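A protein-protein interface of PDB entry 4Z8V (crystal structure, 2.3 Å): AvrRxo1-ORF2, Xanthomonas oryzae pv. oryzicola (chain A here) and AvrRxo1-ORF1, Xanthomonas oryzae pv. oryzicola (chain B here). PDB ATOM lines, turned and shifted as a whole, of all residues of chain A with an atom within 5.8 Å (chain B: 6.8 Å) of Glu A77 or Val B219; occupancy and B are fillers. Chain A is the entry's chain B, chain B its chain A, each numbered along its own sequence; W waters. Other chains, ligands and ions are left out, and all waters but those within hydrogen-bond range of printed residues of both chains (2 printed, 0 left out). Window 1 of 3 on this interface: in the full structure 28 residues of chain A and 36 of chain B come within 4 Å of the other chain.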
ATOM      1  N   ARG A  72     -13.526 -21.727 -29.762  1.00  0.00           N
ATOM      2  CA  ARG A  72     -14.289 -20.551 -30.160  1.00  0.00           C
ATOM      3  C   ARG A  72     -13.516 -19.247 -29.937  1.00  0.00           C
ATOM      4  O   ARG A  72     -13.565 -18.345 -30.771  1.00  0.00           O
ATOM      5  CB  ARG A  72     -15.629 -20.550 -29.432  1.00  0.00           C
ATOM      6  CG  ARG A  72     -16.429 -19.295 -29.575  1.00  0.00           C
ATOM      7  CD  ARG A  72     -17.754 -19.458 -28.864  1.00  0.00           C
ATOM      8  NE  ARG A  72     -18.606 -20.398 -29.581  1.00  0.00           N
ATOM      9  CZ  ARG A  72     -19.350 -20.059 -30.633  1.00  0.00           C
ATOM     10  NH1 ARG A  72     -19.333 -18.800 -31.095  1.00  0.00           N
ATOM     11  NH2 ARG A  72     -20.106 -20.974 -31.228  1.00  0.00           N
ATOM     12  N   MET A  73     -12.782 -19.156 -28.836  1.00  0.00           N
ATOM     13  CA  MET A  73     -11.936 -17.988 -28.583  1.00  0.00           C
ATOM     14  C   MET A  73     -10.822 -17.868 -29.633  1.00  0.00           C
ATOM     15  O   MET A  73     -10.550 -16.786 -30.149  1.00  0.00           O
ATOM     16  CB  MET A  73     -11.332 -18.069 -27.177  1.00  0.00           C
ATOM     17  CG  MET A  73     -10.378 -16.952 -26.854  1.00  0.00           C
ATOM     18  SD  MET A  73      -9.520 -17.150 -25.270  1.00  0.00           S
ATOM     19  CE  MET A  73     -10.899 -17.230 -24.131  1.00  0.00           C
ATOM     20  N   TYR A  74     -10.206 -19.004 -29.955  1.00  0.00           N
ATOM     21  CA  TYR A  74      -9.122 -19.094 -30.928  1.00  0.00           C
ATOM     22  C   TYR A  74      -9.527 -18.583 -32.321  1.00  0.00           C
ATOM     23  O   TYR A  74      -8.796 -17.802 -32.963  1.00  0.00           O
ATOM     24  CB  TYR A  74      -8.675 -20.564 -31.002  1.00  0.00           C
ATOM     25  CG  TYR A  74      -7.580 -20.889 -31.999  1.00  0.00           C
ATOM     26  CD1 TYR A  74      -6.293 -20.383 -31.851  1.00  0.00           C
ATOM     27  CD2 TYR A  74      -7.835 -21.724 -33.079  1.00  0.00           C
ATOM     28  CE1 TYR A  74      -5.296 -20.698 -32.763  1.00  0.00           C
ATOM     29  CE2 TYR A  74      -6.844 -22.050 -33.991  1.00  0.00           C
ATOM     30  CZ  TYR A  74      -5.586 -21.538 -33.829  1.00  0.00           C
ATOM     31  OH  TYR A  74      -4.614 -21.859 -34.739  1.00  0.00           O
ATOM     32  N   TYR A  75     -10.696 -19.029 -32.776  1.00  0.00           N
ATOM     33  CA  TYR A  75     -11.193 -18.663 -34.090  1.00  0.00           C
ATOM     34  C   TYR A  75     -11.941 -17.341 -34.122  1.00  0.00           C
ATOM     35  O   TYR A  75     -11.740 -16.544 -35.031  1.00  0.00           O
ATOM     36  CB  TYR A  75     -12.109 -19.761 -34.621  1.00  0.00           C
ATOM     37  CG  TYR A  75     -11.351 -20.987 -35.060  1.00  0.00           C
ATOM     38  CD1 TYR A  75     -10.402 -20.907 -36.083  1.00  0.00           C
ATOM     39  CD2 TYR A  75     -11.588 -22.224 -34.467  1.00  0.00           C
ATOM     40  CE1 TYR A  75      -9.703 -22.025 -36.500  1.00  0.00           C
ATOM     41  CE2 TYR A  75     -10.900 -23.353 -34.880  1.00  0.00           C
ATOM     42  CZ  TYR A  75      -9.959 -23.244 -35.902  1.00  0.00           C
ATOM     43  OH  TYR A  75      -9.260 -24.346 -36.321  1.00  0.00           O
ATOM     44  N   VAL A  76     -12.825 -17.113 -33.154  1.00  0.00           N
ATOM     45  CA  VAL A  76     -13.681 -15.930 -33.212  1.00  0.00           C
ATOM     46  C   VAL A  76     -13.011 -14.651 -32.684  1.00  0.00           C
ATOM     47  O   VAL A  76     -13.137 -13.597 -33.293  1.00  0.00           O
ATOM     48  CB  VAL A  76     -15.010 -16.174 -32.493  1.00  0.00           C
ATOM     49  CG1 VAL A  76     -15.881 -14.934 -32.542  1.00  0.00           C
ATOM     50  CG2 VAL A  76     -15.725 -17.361 -33.125  1.00  0.00           C
ATOM     51  N   GLU A  77     -12.300 -14.733 -31.560  1.00  0.00           N
ATOM     52  CA  GLU A  77     -11.721 -13.528 -30.965  1.00  0.00           C
ATOM     53  C   GLU A  77     -10.329 -13.190 -31.484  1.00  0.00           C
ATOM     54  O   GLU A  77      -9.906 -12.041 -31.396  1.00  0.00           O
ATOM     55  CB  GLU A  77     -11.666 -13.636 -29.431  1.00  0.00           C
ATOM     56  CG  GLU A  77     -12.993 -13.960 -28.783  1.00  0.00           C
ATOM     57  CD  GLU A  77     -12.915 -13.906 -27.271  1.00  0.00           C
ATOM     58  OE1 GLU A  77     -13.589 -14.726 -26.615  1.00  0.00           O
ATOM     59  OE2 GLU A  77     -12.193 -13.030 -26.735  1.00  0.00           O
ATOM     60  N   TYR A  78      -9.613 -14.157 -31.985  1.00  0.00           N
ATOM     61  CA  TYR A  78      -8.239 -13.945 -32.340  1.00  0.00           C
ATOM     62  C   TYR A  78      -7.924 -14.416 -33.721  1.00  0.00           C
ATOM     63  O   TYR A  78      -7.077 -15.228 -33.908  1.00  0.00           O
ATOM     64  CB  TYR A  78      -7.345 -14.617 -31.306  1.00  0.00           C
ATOM     65  CG  TYR A  78      -7.478 -13.982 -29.950  1.00  0.00           C
ATOM     66  CD1 TYR A  78      -6.865 -12.796 -29.669  1.00  0.00           C
ATOM     67  CD2 TYR A  78      -8.262 -14.532 -28.995  1.00  0.00           C
ATOM     68  CE1 TYR A  78      -6.999 -12.213 -28.495  1.00  0.00           C
ATOM     69  CE2 TYR A  78      -8.393 -13.959 -27.819  1.00  0.00           C
ATOM     70  CZ  TYR A  78      -7.761 -12.793 -27.562  1.00  0.00           C
ATOM     71  OH  TYR A  78      -7.899 -12.195 -26.380  1.00  0.00           O
ATOM     72  N   PRO A  79      -8.636 -13.902 -34.697  1.00  0.00           N
ATOM     73  CA  PRO A  79      -8.549 -14.409 -36.059  1.00  0.00           C
ATOM     74  C   PRO A  79      -7.208 -14.155 -36.727  1.00  0.00           C
ATOM     75  O   PRO A  79      -6.873 -14.843 -37.632  1.00  0.00           O
ATOM     76  CB  PRO A  79      -9.624 -13.628 -36.753  1.00  0.00           C
ATOM     77  CG  PRO A  79      -9.621 -12.408 -36.094  1.00  0.00           C
ATOM     78  CD  PRO A  79      -9.399 -12.665 -34.675  1.00  0.00           C
ATOM     79  N   ASN B  74     -17.834  -7.191 -16.469  1.00  0.00           N
ATOM     80  CA  ASN B  74     -16.443  -7.075 -16.895  1.00  0.00           C
ATOM     81  C   ASN B  74     -15.708  -6.036 -16.046  1.00  0.00           C
ATOM     82  O   ASN B  74     -16.324  -5.236 -15.310  1.00  0.00           O
ATOM     83  CB  ASN B  74     -16.366  -6.701 -18.377  1.00  0.00           C
ATOM     84  CG  ASN B  74     -15.018  -6.999 -18.989  1.00  0.00           C
ATOM     85  OD1 ASN B  74     -14.286  -7.872 -18.515  1.00  0.00           O
ATOM     86  ND2 ASN B  74     -14.672  -6.260 -20.056  1.00  0.00           N
ATOM     87  N   SER B 162     -18.032 -14.404 -15.544  1.00  0.00           N
ATOM     88  CA  SER B 162     -18.412 -14.332 -16.935  1.00  0.00           C
ATOM     89  C   SER B 162     -18.894 -15.682 -17.475  1.00  0.00           C
ATOM     90  O   SER B 162     -19.749 -15.720 -18.360  1.00  0.00           O
ATOM     91  CB  SER B 162     -17.240 -13.829 -17.768  1.00  0.00           C
ATOM     92  OG  SER B 162     -16.306 -14.877 -18.007  1.00  0.00           O
ATOM     93  N   ARG B 163     -18.364 -16.788 -16.953  1.00  0.00           N
ATOM     94  CA  ARG B 163     -18.631 -18.100 -17.560  1.00  0.00           C
ATOM     95  C   ARG B 163     -19.744 -18.891 -16.870  1.00  0.00           C
ATOM     96  O   ARG B 163     -19.987 -18.732 -15.661  1.00  0.00           O
ATOM     97  CB  ARG B 163     -17.348 -18.935 -17.625  1.00  0.00           C
ATOM     98  CG  ARG B 163     -16.158 -18.218 -18.260  1.00  0.00           C
ATOM     99  CD  ARG B 163     -15.881 -18.636 -19.705  1.00  0.00           C
ATOM    100  NE  ARG B 163     -14.763 -17.863 -20.249  1.00  0.00           N
ATOM    101  CZ  ARG B 163     -14.669 -17.442 -21.508  1.00  0.00           C
ATOM    102  NH1 ARG B 163     -15.627 -17.732 -22.382  1.00  0.00           N
ATOM    103  NH2 ARG B 163     -13.612 -16.726 -21.892  1.00  0.00           N
ATOM    104  N   LEU B 190     -17.096  -1.913 -24.265  1.00  0.00           N
ATOM    105  CA  LEU B 190     -15.703  -2.293 -24.131  1.00  0.00           C
ATOM    106  C   LEU B 190     -14.771  -1.092 -23.963  1.00  0.00           C
ATOM    107  O   LEU B 190     -13.865  -1.126 -23.116  1.00  0.00           O
ATOM    108  CB  LEU B 190     -15.279  -3.130 -25.338  1.00  0.00           C
ATOM    109  CG  LEU B 190     -13.846  -3.670 -25.349  1.00  0.00           C
ATOM    110  CD1 LEU B 190     -13.505  -4.259 -24.007  1.00  0.00           C
ATOM    111  CD2 LEU B 190     -13.720  -4.718 -26.434  1.00  0.00           C
ATOM    112  N   PRO B 212      -6.154  -8.156 -23.918  1.00  0.00           N
ATOM    113  CA  PRO B 212      -6.896  -9.401 -24.164  1.00  0.00           C
ATOM    114  C   PRO B 212      -7.727  -9.842 -22.955  1.00  0.00           C
ATOM    115  O   PRO B 212      -8.767 -10.477 -23.125  1.00  0.00           O
ATOM    116  CB  PRO B 212      -5.789 -10.427 -24.445  1.00  0.00           C
ATOM    117  CG  PRO B 212      -4.604  -9.626 -24.880  1.00  0.00           C
ATOM    118  CD  PRO B 212      -4.698  -8.343 -24.089  1.00  0.00           C
ATOM    119  N   VAL B 214      -9.345  -7.755 -20.911  1.00  0.00           N
ATOM    120  CA  VAL B 214     -10.537  -6.919 -20.877  1.00  0.00           C
ATOM    121  C   VAL B 214     -11.486  -7.293 -22.010  1.00  0.00           C
ATOM    122  O   VAL B 214     -12.710  -7.352 -21.820  1.00  0.00           O
ATOM    123  CB  VAL B 214     -10.163  -5.419 -20.958  1.00  0.00           C
ATOM    124  CG1 VAL B 214     -11.417  -4.542 -20.878  1.00  0.00           C
ATOM    125  CG2 VAL B 214      -9.191  -5.056 -19.840  1.00  0.00           C
ATOM    126  N   SER B 215     -10.919  -7.564 -23.181  1.00  0.00           N
ATOM    127  CA  SER B 215     -11.714  -7.882 -24.371  1.00  0.00           C
ATOM    128  C   SER B 215     -12.390  -9.248 -24.280  1.00  0.00           C
ATOM    129  O   SER B 215     -13.566  -9.399 -24.600  1.00  0.00           O
ATOM    130  CB  SER B 215     -10.821  -7.849 -25.610  1.00  0.00           C
ATOM    131  OG  SER B 215     -11.600  -7.978 -26.781  1.00  0.00           O
ATOM    132  N   SER B 216     -11.627 -10.243 -23.859  1.00  0.00           N
ATOM    133  CA  SER B 216     -12.140 -11.582 -23.700  1.00  0.00           C
ATOM    134  C   SER B 216     -13.129 -11.648 -22.558  1.00  0.00           C
ATOM    135  O   SER B 216     -14.095 -12.404 -22.627  1.00  0.00           O
ATOM    136  CB  SER B 216     -10.992 -12.560 -23.479  1.00  0.00           C
ATOM    137  OG  SER B 216     -10.321 -12.733 -24.705  1.00  0.00           O
ATOM    138  N   GLY B 217     -12.902 -10.842 -21.520  1.00  0.00           N
ATOM    139  CA  GLY B 217     -13.868 -10.742 -20.436  1.00  0.00           C
ATOM    140  C   GLY B 217     -15.191 -10.190 -20.934  1.00  0.00           C
ATOM    141  O   GLY B 217     -16.264 -10.723 -20.615  1.00  0.00           O
ATOM    142  N   PHE B 218     -15.107  -9.119 -21.725  1.00  0.00           N
ATOM    143  CA  PHE B 218     -16.269  -8.497 -22.368  1.00  0.00           C
ATOM    144  C   PHE B 218     -17.082  -9.470 -23.240  1.00  0.00           C
ATOM    145  O   PHE B 218     -18.300  -9.544 -23.124  1.00  0.00           O
ATOM    146  CB  PHE B 218     -15.781  -7.321 -23.205  1.00  0.00           C
ATOM    147  CG  PHE B 218     -16.853  -6.655 -24.041  1.00  0.00           C
ATOM    148  CD1 PHE B 218     -17.655  -5.661 -23.500  1.00  0.00           C
ATOM    149  CD2 PHE B 218     -17.013  -6.981 -25.387  1.00  0.00           C
ATOM    150  CE1 PHE B 218     -18.623  -5.027 -24.284  1.00  0.00           C
ATOM    151  CE2 PHE B 218     -17.980  -6.346 -26.171  1.00  0.00           C
ATOM    152  CZ  PHE B 218     -18.779  -5.375 -25.617  1.00  0.00           C
ATOM    153  N   VAL B 219     -16.412 -10.207 -24.114  1.00  0.00           N
ATOM    154  CA  VAL B 219     -17.100 -11.164 -24.973  1.00  0.00           C
ATOM    155  C   VAL B 219     -17.852 -12.215 -24.150  1.00  0.00           C
ATOM    156  O   VAL B 219     -19.010 -12.519 -24.416  1.00  0.00           O
ATOM    157  CB  VAL B 219     -16.119 -11.869 -25.926  1.00  0.00           C
ATOM    158  CG1 VAL B 219     -16.763 -13.141 -26.535  1.00  0.00           C
ATOM    159  CG2 VAL B 219     -15.680 -10.908 -27.030  1.00  0.00           C
ATOM    160  N   ALA B 220     -17.188 -12.742 -23.134  1.00  0.00           N
ATOM    161  CA  ALA B 220     -17.727 -13.833 -22.352  1.00  0.00           C
ATOM    162  C   ALA B 220     -18.894 -13.362 -21.493  1.00  0.00           C
ATOM    163  O   ALA B 220     -19.913 -14.068 -21.384  1.00  0.00           O
ATOM    164  CB  ALA B 220     -16.621 -14.448 -21.475  1.00  0.00           C
ATOM    165  N   VAL B 221     -18.748 -12.191 -20.863  1.00  0.00           N
ATOM    166  CA  VAL B 221     -19.802 -11.716 -19.974  1.00  0.00           C
ATOM    167  C   VAL B 221     -21.065 -11.396 -20.764  1.00  0.00           C
ATOM    168  O   VAL B 221     -22.175 -11.626 -20.288  1.00  0.00           O
ATOM    169  CB  VAL B 221     -19.367 -10.515 -19.102  1.00  0.00           C
ATOM    170  CG1 VAL B 221     -19.381  -9.216 -19.901  1.00  0.00           C
ATOM    171  CG2 VAL B 221     -20.289 -10.383 -17.914  1.00  0.00           C
ATOM    172  N   ARG B 222     -20.890 -10.898 -21.982  1.00  0.00           N
ATOM    173  CA  ARG B 222     -22.018 -10.576 -22.848  1.00  0.00           C
ATOM    174  C   ARG B 222     -22.677 -11.836 -23.406  1.00  0.00           C
ATOM    175  O   ARG B 222     -23.902 -11.947 -23.401  1.00  0.00           O
ATOM    176  CB  ARG B 222     -21.555  -9.671 -24.007  1.00  0.00           C
ATOM    177  CG  ARG B 222     -21.306  -8.221 -23.610  1.00  0.00           C
ATOM    178  CD  ARG B 222     -22.275  -7.307 -24.291  1.00  0.00           C
ATOM    179  NE  ARG B 222     -22.145  -5.910 -23.861  1.00  0.00           N
ATOM    180  CZ  ARG B 222     -22.154  -4.878 -24.697  1.00  0.00           C
ATOM    181  NH1 ARG B 222     -22.260  -5.092 -26.009  1.00  0.00           N
ATOM    182  NH2 ARG B 222     -22.049  -3.645 -24.222  1.00  0.00           N
ATOM    183  N   SER B 223     -21.860 -12.773 -23.891  1.00  0.00           N
ATOM    184  CA  SER B 223     -22.361 -13.999 -24.523  1.00  0.00           C
ATOM    185  C   SER B 223     -23.049 -14.951 -23.542  1.00  0.00           C
ATOM    186  O   SER B 223     -23.903 -15.760 -23.940  1.00  0.00           O
ATOM    187  CB  SER B 223     -21.224 -14.745 -25.228  1.00  0.00           C
ATOM    188  OG  SER B 223     -20.473 -13.870 -26.050  1.00  0.00           O
ATOM    189  N   ASN B 224     -22.683 -14.866 -22.269  1.00  0.00           N
ATOM    190  CA  ASN B 224     -23.278 -15.741 -21.255  1.00  0.00           C
ATOM    191  C   ASN B 224     -24.335 -15.058 -20.385  1.00  0.00           C
ATOM    192  O   ASN B 224     -24.879 -15.653 -19.455  1.00  0.00           O
ATOM    193  CB  ASN B 224     -22.166 -16.357 -20.399  1.00  0.00           C
ATOM    194  CG  ASN B 224     -21.263 -17.251 -21.212  1.00  0.00           C
ATOM    195  OD1 ASN B 224     -21.731 -18.202 -21.839  1.00  0.00           O
ATOM    196  ND2 ASN B 224     -19.977 -16.943 -21.241  1.00  0.00           N
ATOM    197  N   SER B 276     -25.040  -9.355 -26.607  1.00  0.00           N
ATOM    198  CA  SER B 276     -24.129  -9.904 -27.608  1.00  0.00           C
ATOM    199  C   SER B 276     -22.863  -9.063 -27.656  1.00  0.00           C
ATOM    200  O   SER B 276     -22.888  -7.894 -27.283  1.00  0.00           O
ATOM    201  CB  SER B 276     -24.781  -9.940 -28.988  1.00  0.00           C
ATOM    202  OG  SER B 276     -24.720  -8.662 -29.594  1.00  0.00           O
ATOM    203  N   PRO B 277     -21.743  -9.656 -28.111  1.00  0.00           N
ATOM    204  CA  PRO B 277     -20.491  -8.889 -28.038  1.00  0.00           C
ATOM    205  C   PRO B 277     -20.213  -7.996 -29.238  1.00  0.00           C
ATOM    206  O   PRO B 277     -19.192  -7.299 -29.197  1.00  0.00           O
ATOM    207  CB  PRO B 277     -19.427  -9.978 -27.935  1.00  0.00           C
ATOM    208  CG  PRO B 277     -20.026 -11.136 -28.642  1.00  0.00           C
ATOM    209  CD  PRO B 277     -21.500 -11.085 -28.378  1.00  0.00           C
ATOM    210  N   LEU B 279     -19.010  -8.241 -32.372  1.00  0.00           N
ATOM    211  CA  LEU B 279     -17.632  -8.348 -32.855  1.00  0.00           C
ATOM    212  C   LEU B 279     -17.159  -7.266 -33.864  1.00  0.00           C
ATOM    213  O   LEU B 279     -15.956  -7.007 -33.984  1.00  0.00           O
ATOM    214  CB  LEU B 279     -17.354  -9.765 -33.377  1.00  0.00           C
ATOM    215  CG  LEU B 279     -17.256 -10.818 -32.273  1.00  0.00           C
ATOM    216  CD1 LEU B 279     -16.607 -10.240 -31.027  1.00  0.00           C
ATOM    217  CD2 LEU B 279     -18.604 -11.381 -31.918  1.00  0.00           C
HETATM  218  O   HOH W   1     -14.012 -14.754 -24.152  1.00  0.00           O
HETATM  219  O   HOH W   2     -11.574 -10.434 -27.453  1.00  0.00           O
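OH of Tyr A78 is in hydrogen-bond range of OG of Ser B216 (3.0 Å).
The side-chain carboxylate of Glu A77 is in hydrogen-bond range of the side-chain hydroxyl of Ser B216.
The backbone carbonyl oxygen (O) of Met A73 lies within hydrogen-bond range of the backbone NH (N) of Tyr A78.
The backbone carbonyl oxygen (O) of Pro B212 lies close to the side-chain hydroxyl (OG) of Ser B216 (3.2 Å).
O of Val B219 sits at hydrogen-bond distance from OG of Ser B223 (2.6 Å).
Met A73 touches Arg B163 (CE to NH2, 3.6 Å).
Glu A77 touches Val B219 (OE1 to CG1, 3.5 Å).
Pro B212 touches Tyr A78.
Of the printed residues of chain B, Met A73 touches Arg B163 (3.6 Å).
Glu A77 touches two residues of chain B.
Printed residues of chain B within 4 Å of Tyr A78: Pro B212 (3.4 Å) and Ser B216 (3.0 Å).
Val B219 touches just one residue of chain A: Glu A77.
The nearest printed residue of chain A that does not touch Val B219 is Val A76 (6.3 Å).
Hydrophobic or aromatic side chains of chain A within 4 Å of the printed part of chain B: Met A73 and Tyr A78.
Of the 19 printed residues of chain B, 4 touch a printed residue of chain A.
Among the printed residues, 5 pairs touch across the chains.
Water W1 lies within hydrogen-bond range of the side-chain carboxylate of Glu A77 (2.5 Å), the backbone carbonyl oxygen of Ser B216 (2.8 Å) and the guanidinium group of Arg B163 (3.0 Å).
Water W2 lies within hydrogen-bond range of the side-chain hydroxyl of Ser B215 (2.5 Å) and the side-chain carboxylate of Glu A77 (2.8 Å).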
